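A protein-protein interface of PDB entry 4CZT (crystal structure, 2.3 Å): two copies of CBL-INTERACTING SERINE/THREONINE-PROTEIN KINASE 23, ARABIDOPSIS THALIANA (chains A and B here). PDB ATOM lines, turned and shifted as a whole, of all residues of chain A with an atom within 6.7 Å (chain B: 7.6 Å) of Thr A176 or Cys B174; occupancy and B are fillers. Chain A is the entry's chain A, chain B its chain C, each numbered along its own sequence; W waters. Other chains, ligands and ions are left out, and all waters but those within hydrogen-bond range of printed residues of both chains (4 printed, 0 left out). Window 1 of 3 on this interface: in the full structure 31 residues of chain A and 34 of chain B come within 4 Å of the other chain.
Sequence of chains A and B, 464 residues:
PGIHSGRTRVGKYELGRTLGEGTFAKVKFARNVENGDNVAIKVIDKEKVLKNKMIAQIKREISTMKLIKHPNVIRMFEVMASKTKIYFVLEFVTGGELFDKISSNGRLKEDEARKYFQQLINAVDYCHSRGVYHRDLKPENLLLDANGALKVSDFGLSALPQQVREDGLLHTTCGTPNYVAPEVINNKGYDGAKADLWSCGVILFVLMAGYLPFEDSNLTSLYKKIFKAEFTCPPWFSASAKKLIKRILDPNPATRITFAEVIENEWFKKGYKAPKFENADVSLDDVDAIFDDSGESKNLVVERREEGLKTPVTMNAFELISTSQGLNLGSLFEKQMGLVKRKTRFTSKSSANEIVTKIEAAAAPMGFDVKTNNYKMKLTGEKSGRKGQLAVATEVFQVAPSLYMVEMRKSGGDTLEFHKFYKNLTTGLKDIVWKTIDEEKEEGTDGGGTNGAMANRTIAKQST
Of the 18 printed residues of chain A, 7 touch a printed residue of chain B. Hydrophobic or aromatic side chains of chain A that line the printed part of chain B: Leu A170, Tyr A179 and Leu A212. Along chain B the printed residues that touch a printed residue of chain A span positions 99 to 215. Among the printed residues, 14 pairs touch across the chains.
Phe B99 touches Leu A170. CG1 of Val B206 touches CD1 of Leu A170, at 3.9 Å. Glu B215 touches Thr A173 (OE1 to CG2, 3.5 Å). Leu B212 touches Cys A174. Gly A175 touches Gly B175. Cys B174 touches Thr A176 (CA to OG1, 3.7 Å). OG1 of Thr B176 touches CG2 of Thr A176 (3.8 Å). CD1 of Leu A212 touches O of His B171 (3.3 Å).
Water W1 lies within hydrogen-bond range of the backbone NH (N) of Leu A212 and the backbone NH (N) of His B171. Water W3 lies within hydrogen-bond range of the backbone NH (N) of Leu B212 (2.9 Å), the side-chain carboxylate (OE2) of Glu B215 (2.9 Å) and the backbone carbonyl oxygen (O) of Thr A173 (3.5 Å). Water W2 lies within hydrogen-bond range of N of Thr B173 (3.0 Å), OD1 of Asn A178 (3.1 Å) and OG1 of Thr B176 (3.4 Å). Water W4 lies within hydrogen-bond range of O of Cys A174 (3.2 Å) and ND2 of Asn B178 (3.3 Å).
OG1 of Thr B173 is in hydrogen-bond range of OE1 of Glu B140 (2.7 Å). O of Thr B173 is in hydrogen-bond range of OG1 of Thr B176. ND2 of Asn B178 sits close to O of Gly B175 (3.4 Å). N of Leu B212 sits at hydrogen-bond distance from OE2 of Glu B215 (3.4 Å).
The side-chain sulfur (SG) of Cys A174 forms a disulfide with the side-chain sulfur (SG) of Cys B174 (2.1 Å). O of Cys A174 lies close to N of Gly B175 (3.3 Å). OG1 of Thr A176 is in hydrogen-bond range of O of Thr B173, at 2.7 Å. The side-chain hydroxyl (OG1) of Thr A176 lies within hydrogen-bond range of the backbone NH (N) of Gly B175, 3.2 Å away. The side-chain hydroxyl of Thr B172 lies within hydrogen-bond range of the side-chain hydroxyl of Tyr A179, at 3.0 Å. O of Thr A173 sits close to SG of Cys B174.
Thr A173 touches Cys B174, but with the chains exchanged Cys A174 does not touch Thr B173 (5.5 Å). Cys B174 touches its own counterpart, Cys A174. Cys A174 touches Gly B175, but with the chains exchanged Gly A175 does not touch Cys B174 (5.5 Å). Tyr A179 touches Thr B172, but with the chains exchanged Thr A172 does not touch Tyr B179 (12.5 Å). 14 positions are printed for both chains.
Of the printed residues of chain B, Leu A170 touches Phe B99 and Val B206. Printed residues of chain B within 4 Å of Thr A173: Cys B174 and Glu B215. Printed residues of chain B within 4 Å of Cys A174: Cys B174, Gly B175 and Leu B212. Thr A176 touches just these residues of chain B: Thr B173 (2.7 Å), Cys B174 (3.7 Å), Gly B175 (3.2 Å) and Thr B176 (3.8 Å). Pro A177 touches none of the printed residues of chain B. Of the printed residues of chain A, Phe B99 touches Leu A170 (3.6 Å). Printed residues of chain A within 4 Å of Thr B176: Thr A176. Leu B222 touches none of the printed residues of chain A. The nearest residue of chain B that does not touch Thr A176 is Thr B172 (4.6 Å). The nearest residue of chain A that does not touch Cys B174 is Leu A170 (4.2 Å).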
ATOM      1  N   ASP A 136     -24.078   9.259  -9.566  1.00  0.00           N
ATOM      2  CA  ASP A 136     -23.995   7.853  -9.173  1.00  0.00           C
ATOM      3  C   ASP A 136     -22.828   7.575  -8.204  1.00  0.00           C
ATOM      4  O   ASP A 136     -22.202   6.519  -8.274  1.00  0.00           O
ATOM      5  CB  ASP A 136     -23.886   6.974 -10.425  1.00  0.00           C
ATOM      6  CG  ASP A 136     -24.258   5.510 -10.161  1.00  0.00           C
ATOM      7  OD1 ASP A 136     -25.032   5.226  -9.215  1.00  0.00           O
ATOM      8  OD2 ASP A 136     -23.777   4.636 -10.912  1.00  0.00           O
ATOM      9  N   LEU A 137     -22.535   8.517  -7.304  1.00  0.00           N
ATOM     10  CA  LEU A 137     -21.378   8.363  -6.414  1.00  0.00           C
ATOM     11  C   LEU A 137     -21.553   7.168  -5.483  1.00  0.00           C
ATOM     12  O   LEU A 137     -22.555   7.039  -4.782  1.00  0.00           O
ATOM     13  CB  LEU A 137     -21.123   9.634  -5.603  1.00  0.00           C
ATOM     14  CG  LEU A 137     -20.392  10.753  -6.360  1.00  0.00           C
ATOM     15  CD1 LEU A 137     -20.317  12.018  -5.510  1.00  0.00           C
ATOM     16  CD2 LEU A 137     -18.986  10.322  -6.860  1.00  0.00           C
ATOM     17  N   LYS A 138     -20.567   6.284  -5.505  1.00  0.00           N
ATOM     18  CA  LYS A 138     -20.619   5.045  -4.756  1.00  0.00           C
ATOM     19  C   LYS A 138     -19.177   4.612  -4.437  1.00  0.00           C
ATOM     20  O   LYS A 138     -18.236   5.214  -4.957  1.00  0.00           O
ATOM     21  CB  LYS A 138     -21.393   3.981  -5.553  1.00  0.00           C
ATOM     22  CG  LYS A 138     -20.869   3.692  -6.935  1.00  0.00           C
ATOM     23  CD  LYS A 138     -21.860   2.788  -7.666  1.00  0.00           C
ATOM     24  CE  LYS A 138     -21.481   2.581  -9.111  1.00  0.00           C
ATOM     25  NZ  LYS A 138     -21.478   3.881  -9.817  1.00  0.00           N
ATOM     26  N   PRO A 139     -19.002   3.589  -3.572  1.00  0.00           N
ATOM     27  CA  PRO A 139     -17.637   3.151  -3.252  1.00  0.00           C
ATOM     28  C   PRO A 139     -16.837   2.685  -4.471  1.00  0.00           C
ATOM     29  O   PRO A 139     -15.629   2.893  -4.507  1.00  0.00           O
ATOM     30  CB  PRO A 139     -17.842   1.966  -2.296  1.00  0.00           C
ATOM     31  CG  PRO A 139     -19.266   2.046  -1.838  1.00  0.00           C
ATOM     32  CD  PRO A 139     -20.032   2.780  -2.877  1.00  0.00           C
ATOM     33  N   GLU A 140     -17.487   2.041  -5.434  1.00  0.00           N
ATOM     34  CA  GLU A 140     -16.777   1.549  -6.612  1.00  0.00           C
ATOM     35  C   GLU A 140     -16.165   2.678  -7.451  1.00  0.00           C
ATOM     36  O   GLU A 140     -15.341   2.412  -8.314  1.00  0.00           O
ATOM     37  CB  GLU A 140     -17.700   0.711  -7.482  1.00  0.00           C
ATOM     38  CG  GLU A 140     -18.085  -0.624  -6.872  1.00  0.00           C
ATOM     39  CD  GLU A 140     -19.004  -0.489  -5.651  1.00  0.00           C
ATOM     40  OE1 GLU A 140     -19.610   0.595  -5.468  1.00  0.00           O
ATOM     41  OE2 GLU A 140     -19.111  -1.468  -4.868  1.00  0.00           O
ATOM     42  N   LEU A 170     -18.164  -5.062 -12.522  1.00  0.00           N
ATOM     43  CA  LEU A 170     -18.886  -4.724 -11.287  1.00  0.00           C
ATOM     44  C   LEU A 170     -18.428  -3.423 -10.638  1.00  0.00           C
ATOM     45  O   LEU A 170     -18.341  -3.327  -9.420  1.00  0.00           O
ATOM     46  CB  LEU A 170     -18.774  -5.854 -10.264  1.00  0.00           C
ATOM     47  CG  LEU A 170     -19.544  -7.137 -10.587  1.00  0.00           C
ATOM     48  CD1 LEU A 170     -19.349  -8.122  -9.462  1.00  0.00           C
ATOM     49  CD2 LEU A 170     -21.027  -6.847 -10.803  1.00  0.00           C
ATOM     50  N   HIS A 171     -18.143  -2.415 -11.450  1.00  0.00           N
ATOM     51  CA  HIS A 171     -17.751  -1.129 -10.907  1.00  0.00           C
ATOM     52  C   HIS A 171     -18.687  -0.012 -11.318  1.00  0.00           C
ATOM     53  O   HIS A 171     -19.165   0.745 -10.476  1.00  0.00           O
ATOM     54  CB  HIS A 171     -16.319  -0.792 -11.318  1.00  0.00           C
ATOM     55  CG  HIS A 171     -15.292  -1.351 -10.388  1.00  0.00           C
ATOM     56  ND1 HIS A 171     -14.728  -2.596 -10.565  1.00  0.00           N
ATOM     57  CD2 HIS A 171     -14.758  -0.853  -9.248  1.00  0.00           C
ATOM     58  CE1 HIS A 171     -13.874  -2.831  -9.584  1.00  0.00           C
ATOM     59  NE2 HIS A 171     -13.876  -1.790  -8.770  1.00  0.00           N
ATOM     60  N   THR A 172     -18.969   0.088 -12.608  1.00  0.00           N
ATOM     61  CA  THR A 172     -19.612   1.283 -13.112  1.00  0.00           C
ATOM     62  C   THR A 172     -21.121   1.283 -12.866  1.00  0.00           C
ATOM     63  O   THR A 172     -21.718   2.348 -12.713  1.00  0.00           O
ATOM     64  CB  THR A 172     -19.309   1.485 -14.624  1.00  0.00           C
ATOM     65  OG1 THR A 172     -19.840   2.748 -15.040  1.00  0.00           O
ATOM     66  CG2 THR A 172     -19.875   0.334 -15.492  1.00  0.00           C
ATOM     67  N   THR A 173     -21.724   0.100 -12.792  1.00  0.00           N
ATOM     68  CA  THR A 173     -23.172  -0.020 -12.662  1.00  0.00           C
ATOM     69  C   THR A 173     -23.550  -0.844 -11.452  1.00  0.00           C
ATOM     70  O   THR A 173     -23.421  -2.066 -11.450  1.00  0.00           O
ATOM     71  CB  THR A 173     -23.823  -0.683 -13.898  1.00  0.00           C
ATOM     72  OG1 THR A 173     -23.688   0.171 -15.037  1.00  0.00           O
ATOM     73  CG2 THR A 173     -25.305  -0.941 -13.645  1.00  0.00           C
ATOM     74  N   CYS A 174     -24.038  -0.184 -10.419  1.00  0.00           N
ATOM     75  CA  CYS A 174     -24.403  -0.932  -9.247  1.00  0.00           C
ATOM     76  C   CYS A 174     -25.864  -0.710  -8.921  1.00  0.00           C
ATOM     77  O   CYS A 174     -26.639  -1.665  -8.908  1.00  0.00           O
ATOM     78  CB  CYS A 174     -23.462  -0.580  -8.098  1.00  0.00           C
ATOM     79  SG  CYS A 174     -21.810  -1.336  -8.424  1.00  0.00           S
ATOM     80  N   GLY A 175     -26.266   0.540  -8.732  1.00  0.00           N
ATOM     81  CA  GLY A 175     -27.648   0.800  -8.382  1.00  0.00           C
ATOM     82  C   GLY A 175     -27.907   0.269  -6.984  1.00  0.00           C
ATOM     83  O   GLY A 175     -28.685  -0.672  -6.779  1.00  0.00           O
ATOM     84  N   THR A 176     -27.209   0.870  -6.029  1.00  0.00           N
ATOM     85  CA  THR A 176     -27.341   0.553  -4.619  1.00  0.00           C
ATOM     86  C   THR A 176     -27.989   1.733  -3.907  1.00  0.00           C
ATOM     87  O   THR A 176     -27.405   2.808  -3.867  1.00  0.00           O
ATOM     88  CB  THR A 176     -25.963   0.249  -4.005  1.00  0.00           C
ATOM     89  OG1 THR A 176     -25.369  -0.859  -4.701  1.00  0.00           O
ATOM     90  CG2 THR A 176     -26.082  -0.057  -2.525  1.00  0.00           C
ATOM     91  N   PRO A 177     -29.202   1.539  -3.353  1.00  0.00           N
ATOM     92  CA  PRO A 177     -29.970   2.638  -2.750  1.00  0.00           C
ATOM     93  C   PRO A 177     -29.277   3.306  -1.537  1.00  0.00           C
ATOM     94  O   PRO A 177     -29.531   4.472  -1.249  1.00  0.00           O
ATOM     95  CB  PRO A 177     -31.281   1.961  -2.329  1.00  0.00           C
ATOM     96  CG  PRO A 177     -30.985   0.543  -2.247  1.00  0.00           C
ATOM     97  CD  PRO A 177     -29.901   0.252  -3.232  1.00  0.00           C
ATOM     98  N   ASN A 178     -28.395   2.589  -0.857  1.00  0.00           N
ATOM     99  CA  ASN A 178     -27.781   3.135   0.353  1.00  0.00           C
ATOM    100  C   ASN A 178     -27.091   4.495   0.168  1.00  0.00           C
ATOM    101  O   ASN A 178     -27.082   5.300   1.087  1.00  0.00           O
ATOM    102  CB  ASN A 178     -26.792   2.133   0.918  1.00  0.00           C
ATOM    103  CG  ASN A 178     -27.422   0.773   1.136  1.00  0.00           C
ATOM    104  OD1 ASN A 178     -27.566  -0.002   0.198  1.00  0.00           O
ATOM    105  ND2 ASN A 178     -27.804   0.478   2.380  1.00  0.00           N
ATOM    106  N   TYR A 179     -26.553   4.760  -1.026  1.00  0.00           N
ATOM    107  CA  TYR A 179     -25.858   6.019  -1.296  1.00  0.00           C
ATOM    108  C   TYR A 179     -26.730   7.052  -2.022  1.00  0.00           C
ATOM    109  O   TYR A 179     -26.282   8.157  -2.291  1.00  0.00           O
ATOM    110  CB  TYR A 179     -24.571   5.738  -2.108  1.00  0.00           C
ATOM    111  CG  TYR A 179     -23.707   4.716  -1.416  1.00  0.00           C
ATOM    112  CD1 TYR A 179     -22.851   5.098  -0.405  1.00  0.00           C
ATOM    113  CD2 TYR A 179     -23.797   3.361  -1.724  1.00  0.00           C
ATOM    114  CE1 TYR A 179     -22.089   4.170   0.283  1.00  0.00           C
ATOM    115  CE2 TYR A 179     -23.034   2.429  -1.050  1.00  0.00           C
ATOM    116  CZ  TYR A 179     -22.189   2.841  -0.035  1.00  0.00           C
ATOM    117  OH  TYR A 179     -21.404   1.939   0.662  1.00  0.00           O
ATOM    118  N   VAL A 180     -27.967   6.701  -2.343  1.00  0.00           N
ATOM    119  CA  VAL A 180     -28.801   7.554  -3.187  1.00  0.00           C
ATOM    120  C   VAL A 180     -29.695   8.493  -2.371  1.00  0.00           C
ATOM    121  O   VAL A 180     -30.336   8.074  -1.422  1.00  0.00           O
ATOM    122  CB  VAL A 180     -29.686   6.699  -4.118  1.00  0.00           C
ATOM    123  CG1 VAL A 180     -30.507   7.591  -5.054  1.00  0.00           C
ATOM    124  CG2 VAL A 180     -28.830   5.726  -4.928  1.00  0.00           C
ATOM    125  N   LEU A 212     -22.432   1.974   7.303  1.00  0.00           N
ATOM    126  CA  LEU A 212     -23.413   2.812   6.612  1.00  0.00           C
ATOM    127  C   LEU A 212     -24.394   3.397   7.603  1.00  0.00           C
ATOM    128  O   LEU A 212     -24.739   2.750   8.578  1.00  0.00           O
ATOM    129  CB  LEU A 212     -24.175   2.005   5.558  1.00  0.00           C
ATOM    130  CG  LEU A 212     -23.421   1.464   4.354  1.00  0.00           C
ATOM    131  CD1 LEU A 212     -24.288   0.445   3.646  1.00  0.00           C
ATOM    132  CD2 LEU A 212     -23.077   2.625   3.431  1.00  0.00           C
ATOM    133  N   LEU A 222     -35.195  -0.375   4.503  1.00  0.00           N
ATOM    134  CA  LEU A 222     -34.065   0.403   4.001  1.00  0.00           C
ATOM    135  C   LEU A 222     -34.553   1.726   3.374  1.00  0.00           C
ATOM    136  O   LEU A 222     -34.105   2.804   3.767  1.00  0.00           O
ATOM    137  CB  LEU A 222     -33.250  -0.426   2.990  1.00  0.00           C
ATOM    138  CG  LEU A 222     -32.061   0.277   2.318  1.00  0.00           C
ATOM    139  CD1 LEU A 222     -31.192   0.977   3.369  1.00  0.00           C
ATOM    140  CD2 LEU A 222     -31.216  -0.700   1.514  1.00  0.00           C
ATOM    141  N   PHE B  99     -16.028 -12.277  -5.034  1.00  0.00           N
ATOM    142  CA  PHE B  99     -16.290 -11.361  -6.138  1.00  0.00           C
ATOM    143  C   PHE B  99     -15.075 -10.480  -6.463  1.00  0.00           C
ATOM    144  O   PHE B  99     -15.053  -9.819  -7.499  1.00  0.00           O
ATOM    145  CB  PHE B  99     -17.531 -10.507  -5.859  1.00  0.00           C
ATOM    146  CG  PHE B  99     -18.826 -11.161  -6.297  1.00  0.00           C
ATOM    147  CD1 PHE B  99     -18.979 -12.545  -6.250  1.00  0.00           C
ATOM    148  CD2 PHE B  99     -19.883 -10.396  -6.769  1.00  0.00           C
ATOM    149  CE1 PHE B  99     -20.179 -13.163  -6.667  1.00  0.00           C
ATOM    150  CE2 PHE B  99     -21.085 -10.994  -7.186  1.00  0.00           C
ATOM    151  CZ  PHE B  99     -21.235 -12.380  -7.135  1.00  0.00           C
ATOM    152  N   LYS B 138     -25.789 -12.599   0.070  1.00  0.00           N
ATOM    153  CA  LYS B 138     -25.221 -11.539  -0.748  1.00  0.00           C
ATOM    154  C   LYS B 138     -23.795 -11.951  -1.145  1.00  0.00           C
ATOM    155  O   LYS B 138     -23.223 -12.850  -0.511  1.00  0.00           O
ATOM    156  CB  LYS B 138     -25.216 -10.208   0.020  1.00  0.00           C
ATOM    157  CG  LYS B 138     -26.590  -9.693   0.471  1.00  0.00           C
ATOM    158  CD  LYS B 138     -27.405  -9.177  -0.715  1.00  0.00           C
ATOM    159  CE  LYS B 138     -28.633  -8.383  -0.279  1.00  0.00           C
ATOM    160  NZ  LYS B 138     -29.714  -9.221   0.328  1.00  0.00           N
ATOM    161  N   PRO B 139     -23.218 -11.318  -2.194  1.00  0.00           N
ATOM    162  CA  PRO B 139     -21.809 -11.595  -2.534  1.00  0.00           C
ATOM    163  C   PRO B 139     -20.866 -11.447  -1.341  1.00  0.00           C
ATOM    164  O   PRO B 139     -19.903 -12.200  -1.239  1.00  0.00           O
ATOM    165  CB  PRO B 139     -21.480 -10.547  -3.600  1.00  0.00           C
ATOM    166  CG  PRO B 139     -22.805 -10.231  -4.240  1.00  0.00           C
ATOM    167  CD  PRO B 139     -23.848 -10.388  -3.152  1.00  0.00           C
ATOM    168  N   GLU B 140     -21.164 -10.530  -0.433  1.00  0.00           N
ATOM    169  CA  GLU B 140     -20.291 -10.288   0.707  1.00  0.00           C
ATOM    170  C   GLU B 140     -20.298 -11.464   1.707  1.00  0.00           C
ATOM    171  O   GLU B 140     -19.504 -11.480   2.638  1.00  0.00           O
ATOM    172  CB  GLU B 140     -20.683  -8.980   1.414  1.00  0.00           C
ATOM    173  CG  GLU B 140     -21.780  -9.157   2.456  1.00  0.00           C
ATOM    174  CD  GLU B 140     -22.844  -8.054   2.409  1.00  0.00           C
ATOM    175  OE1 GLU B 140     -22.794  -7.204   1.486  1.00  0.00           O
ATOM    176  OE2 GLU B 140     -23.744  -8.050   3.287  1.00  0.00           O
ATOM    177  N   HIS B 171     -21.296  -3.215   5.567  1.00  0.00           N
ATOM    178  CA  HIS B 171     -22.032  -4.163   4.726  1.00  0.00           C
ATOM    179  C   HIS B 171     -22.551  -3.465   3.495  1.00  0.00           C
ATOM    180  O   HIS B 171     -23.593  -2.818   3.538  1.00  0.00           O
ATOM    181  CB  HIS B 171     -23.217  -4.793   5.465  1.00  0.00           C
ATOM    182  CG  HIS B 171     -22.890  -5.245   6.848  1.00  0.00           C
ATOM    183  ND1 HIS B 171     -23.235  -4.516   7.966  1.00  0.00           N
ATOM    184  CD2 HIS B 171     -22.236  -6.342   7.296  1.00  0.00           C
ATOM    185  CE1 HIS B 171     -22.810  -5.150   9.047  1.00  0.00           C
ATOM    186  NE2 HIS B 171     -22.202  -6.261   8.667  1.00  0.00           N
ATOM    187  N   THR B 172     -21.846  -3.585   2.385  1.00  0.00           N
ATOM    188  CA  THR B 172     -22.346  -2.936   1.188  1.00  0.00           C
ATOM    189  C   THR B 172     -22.348  -3.935   0.030  1.00  0.00           C
ATOM    190  O   THR B 172     -21.488  -4.813  -0.050  1.00  0.00           O
ATOM    191  CB  THR B 172     -21.527  -1.655   0.867  1.00  0.00           C
ATOM    192  OG1 THR B 172     -22.252  -0.827  -0.052  1.00  0.00           O
ATOM    193  CG2 THR B 172     -20.124  -1.993   0.329  1.00  0.00           C
ATOM    194  N   THR B 173     -23.350  -3.826  -0.833  1.00  0.00           N
ATOM    195  CA  THR B 173     -23.520  -4.766  -1.941  1.00  0.00           C
ATOM    196  C   THR B 173     -23.745  -3.984  -3.237  1.00  0.00           C
ATOM    197  O   THR B 173     -24.525  -3.034  -3.253  1.00  0.00           O
ATOM    198  CB  THR B 173     -24.723  -5.736  -1.689  1.00  0.00           C
ATOM    199  OG1 THR B 173     -24.476  -6.528  -0.517  1.00  0.00           O
ATOM    200  CG2 THR B 173     -24.977  -6.667  -2.895  1.00  0.00           C
ATOM    201  N   CYS B 174     -23.061  -4.360  -4.314  1.00  0.00           N
ATOM    202  CA  CYS B 174     -23.339  -3.755  -5.610  1.00  0.00           C
ATOM    203  C   CYS B 174     -24.612  -4.396  -6.136  1.00  0.00           C
ATOM    204  O   CYS B 174     -24.647  -5.605  -6.303  1.00  0.00           O
ATOM    205  CB  CYS B 174     -22.166  -3.950  -6.585  1.00  0.00           C
ATOM    206  SG  CYS B 174     -22.385  -3.307  -8.306  1.00  0.00           S
ATOM    207  N   GLY B 175     -25.658  -3.602  -6.357  1.00  0.00           N
ATOM    208  CA  GLY B 175     -26.907  -4.105  -6.917  1.00  0.00           C
ATOM    209  C   GLY B 175     -27.768  -4.957  -5.991  1.00  0.00           C
ATOM    210  O   GLY B 175     -28.289  -6.003  -6.392  1.00  0.00           O
ATOM    211  N   THR B 176     -27.917  -4.486  -4.757  1.00  0.00           N
ATOM    212  CA  THR B 176     -28.668  -5.163  -3.696  1.00  0.00           C
ATOM    213  C   THR B 176     -29.988  -5.836  -4.111  1.00  0.00           C
ATOM    214  O   THR B 176     -30.167  -7.022  -3.833  1.00  0.00           O
ATOM    215  CB  THR B 176     -28.982  -4.172  -2.554  1.00  0.00           C
ATOM    216  OG1 THR B 176     -27.804  -3.419  -2.251  1.00  0.00           O
ATOM    217  CG2 THR B 176     -29.478  -4.916  -1.318  1.00  0.00           C
ATOM    218  N   PRO B 177     -30.905  -5.100  -4.785  1.00  0.00           N
ATOM    219  CA  PRO B 177     -32.204  -5.703  -5.100  1.00  0.00           C
ATOM    220  C   PRO B 177     -32.106  -6.970  -5.945  1.00  0.00           C
ATOM    221  O   PRO B 177     -32.989  -7.816  -5.836  1.00  0.00           O
ATOM    222  CB  PRO B 177     -32.923  -4.597  -5.884  1.00  0.00           C
ATOM    223  CG  PRO B 177     -32.268  -3.355  -5.457  1.00  0.00           C
ATOM    224  CD  PRO B 177     -30.845  -3.701  -5.258  1.00  0.00           C
ATOM    225  N   ASN B 178     -31.074  -7.091  -6.774  1.00  0.00           N
ATOM    226  CA  ASN B 178     -30.889  -8.301  -7.570  1.00  0.00           C
ATOM    227  C   ASN B 178     -30.891  -9.588  -6.749  1.00  0.00           C
ATOM    228  O   ASN B 178     -31.365 -10.626  -7.215  1.00  0.00           O
ATOM    229  CB  ASN B 178     -29.580  -8.240  -8.347  1.00  0.00           C
ATOM    230  CG  ASN B 178     -29.698  -7.432  -9.608  1.00  0.00           C
ATOM    231  OD1 ASN B 178     -29.662  -7.977 -10.707  1.00  0.00           O
ATOM    232  ND2 ASN B 178     -29.817  -6.121  -9.463  1.00  0.00           N
ATOM    233  N   TYR B 179     -30.355  -9.532  -5.535  1.00  0.00           N
ATOM    234  CA  TYR B 179     -30.164 -10.759  -4.778  1.00  0.00           C
ATOM    235  C   TYR B 179     -31.415 -11.130  -3.987  1.00  0.00           C
ATOM    236  O   TYR B 179     -31.514 -12.237  -3.459  1.00  0.00           O
ATOM    237  CB  TYR B 179     -28.917 -10.627  -3.885  1.00  0.00           C
ATOM    238  CG  TYR B 179     -27.682 -10.421  -4.742  1.00  0.00           C
ATOM    239  CD1 TYR B 179     -27.085 -11.495  -5.420  1.00  0.00           C
ATOM    240  CD2 TYR B 179     -27.143  -9.155  -4.926  1.00  0.00           C
ATOM    241  CE1 TYR B 179     -25.960 -11.293  -6.238  1.00  0.00           C
ATOM    242  CE2 TYR B 179     -26.035  -8.949  -5.752  1.00  0.00           C
ATOM    243  CZ  TYR B 179     -25.453 -10.006  -6.391  1.00  0.00           C
ATOM    244  OH  TYR B 179     -24.361  -9.780  -7.183  1.00  0.00           O
ATOM    245  N   VAL B 206     -23.956 -13.638 -12.092  1.00  0.00           N
ATOM    246  CA  VAL B 206     -22.951 -12.614 -12.011  1.00  0.00           C
ATOM    247  C   VAL B 206     -21.562 -13.199 -12.237  1.00  0.00           C
ATOM    248  O   VAL B 206     -20.759 -12.610 -12.978  1.00  0.00           O
ATOM    249  CB  VAL B 206     -23.004 -11.890 -10.660  1.00  0.00           C
ATOM    250  CG1 VAL B 206     -21.906 -10.820 -10.580  1.00  0.00           C
ATOM    251  CG2 VAL B 206     -24.381 -11.245 -10.460  1.00  0.00           C
ATOM    252  N   LEU B 212     -24.684  -7.683 -13.265  1.00  0.00           N
ATOM    253  CA  LEU B 212     -25.999  -8.022 -12.749  1.00  0.00           C
ATOM    254  C   LEU B 212     -27.030  -8.258 -13.856  1.00  0.00           C
ATOM    255  O   LEU B 212     -26.992  -7.627 -14.914  1.00  0.00           O
ATOM    256  CB  LEU B 212     -26.476  -6.920 -11.816  1.00  0.00           C
ATOM    257  CG  LEU B 212     -25.539  -6.644 -10.652  1.00  0.00           C
ATOM    258  CD1 LEU B 212     -25.740  -5.210 -10.148  1.00  0.00           C
ATOM    259  CD2 LEU B 212     -25.769  -7.672  -9.556  1.00  0.00           C
ATOM    260  N   GLU B 215     -30.634  -4.513 -14.405  1.00  0.00           N
ATOM    261  CA  GLU B 215     -30.111  -3.163 -14.350  1.00  0.00           C
ATOM    262  C   GLU B 215     -31.144  -2.263 -15.018  1.00  0.00           C
ATOM    263  O   GLU B 215     -31.762  -2.624 -16.030  1.00  0.00           O
ATOM    264  CB  GLU B 215     -28.742  -3.061 -15.039  1.00  0.00           C
ATOM    265  CG  GLU B 215     -27.722  -4.099 -14.574  1.00  0.00           C
ATOM    266  CD  GLU B 215     -26.357  -3.983 -15.271  1.00  0.00           C
ATOM    267  OE1 GLU B 215     -26.194  -3.124 -16.168  1.00  0.00           O
ATOM    268  OE2 GLU B 215     -25.439  -4.756 -14.916  1.00  0.00           O
ATOM    269  N   LEU B 219     -36.274   2.986 -11.312  1.00  0.00           N
ATOM    270  CA  LEU B 219     -36.541   2.023 -10.254  1.00  0.00           C
ATOM    271  C   LEU B 219     -37.843   1.240 -10.483  1.00  0.00           C
ATOM    272  O   LEU B 219     -37.905   0.051 -10.179  1.00  0.00           O
ATOM    273  CB  LEU B 219     -36.579   2.718  -8.899  1.00  0.00           C
ATOM    274  CG  LEU B 219     -35.220   3.196  -8.377  1.00  0.00           C
ATOM    275  CD1 LEU B 219     -35.296   3.625  -6.900  1.00  0.00           C
ATOM    276  CD2 LEU B 219     -34.183   2.109  -8.566  1.00  0.00           C
ATOM    277  N   LEU B 222     -36.998  -1.232 -12.923  1.00  0.00           N
ATOM    278  CA  LEU B 222     -36.091  -2.198 -12.330  1.00  0.00           C
ATOM    279  C   LEU B 222     -36.889  -3.265 -11.595  1.00  0.00           C
ATOM    280  O   LEU B 222     -36.727  -4.470 -11.836  1.00  0.00           O
ATOM    281  CB  LEU B 222     -35.108  -1.518 -11.376  1.00  0.00           C
ATOM    282  CG  LEU B 222     -34.127  -2.415 -10.588  1.00  0.00           C
ATOM    283  CD1 LEU B 222     -33.190  -3.253 -11.510  1.00  0.00           C
ATOM    284  CD2 LEU B 222     -33.294  -1.544  -9.684  1.00  0.00           C
HETATM  285  O   HOH W   1     -22.533  -0.910   7.009  1.00  0.00           O
HETATM  286  O   HOH W   2     -25.785  -2.557   0.342  1.00  0.00           O
HETATM  287  O   HOH W   3     -23.272  -5.158 -12.984  1.00  0.00           O
HETATM  288  O   HOH W   4     -29.004  -3.049 -10.519  1.00  0.00           O
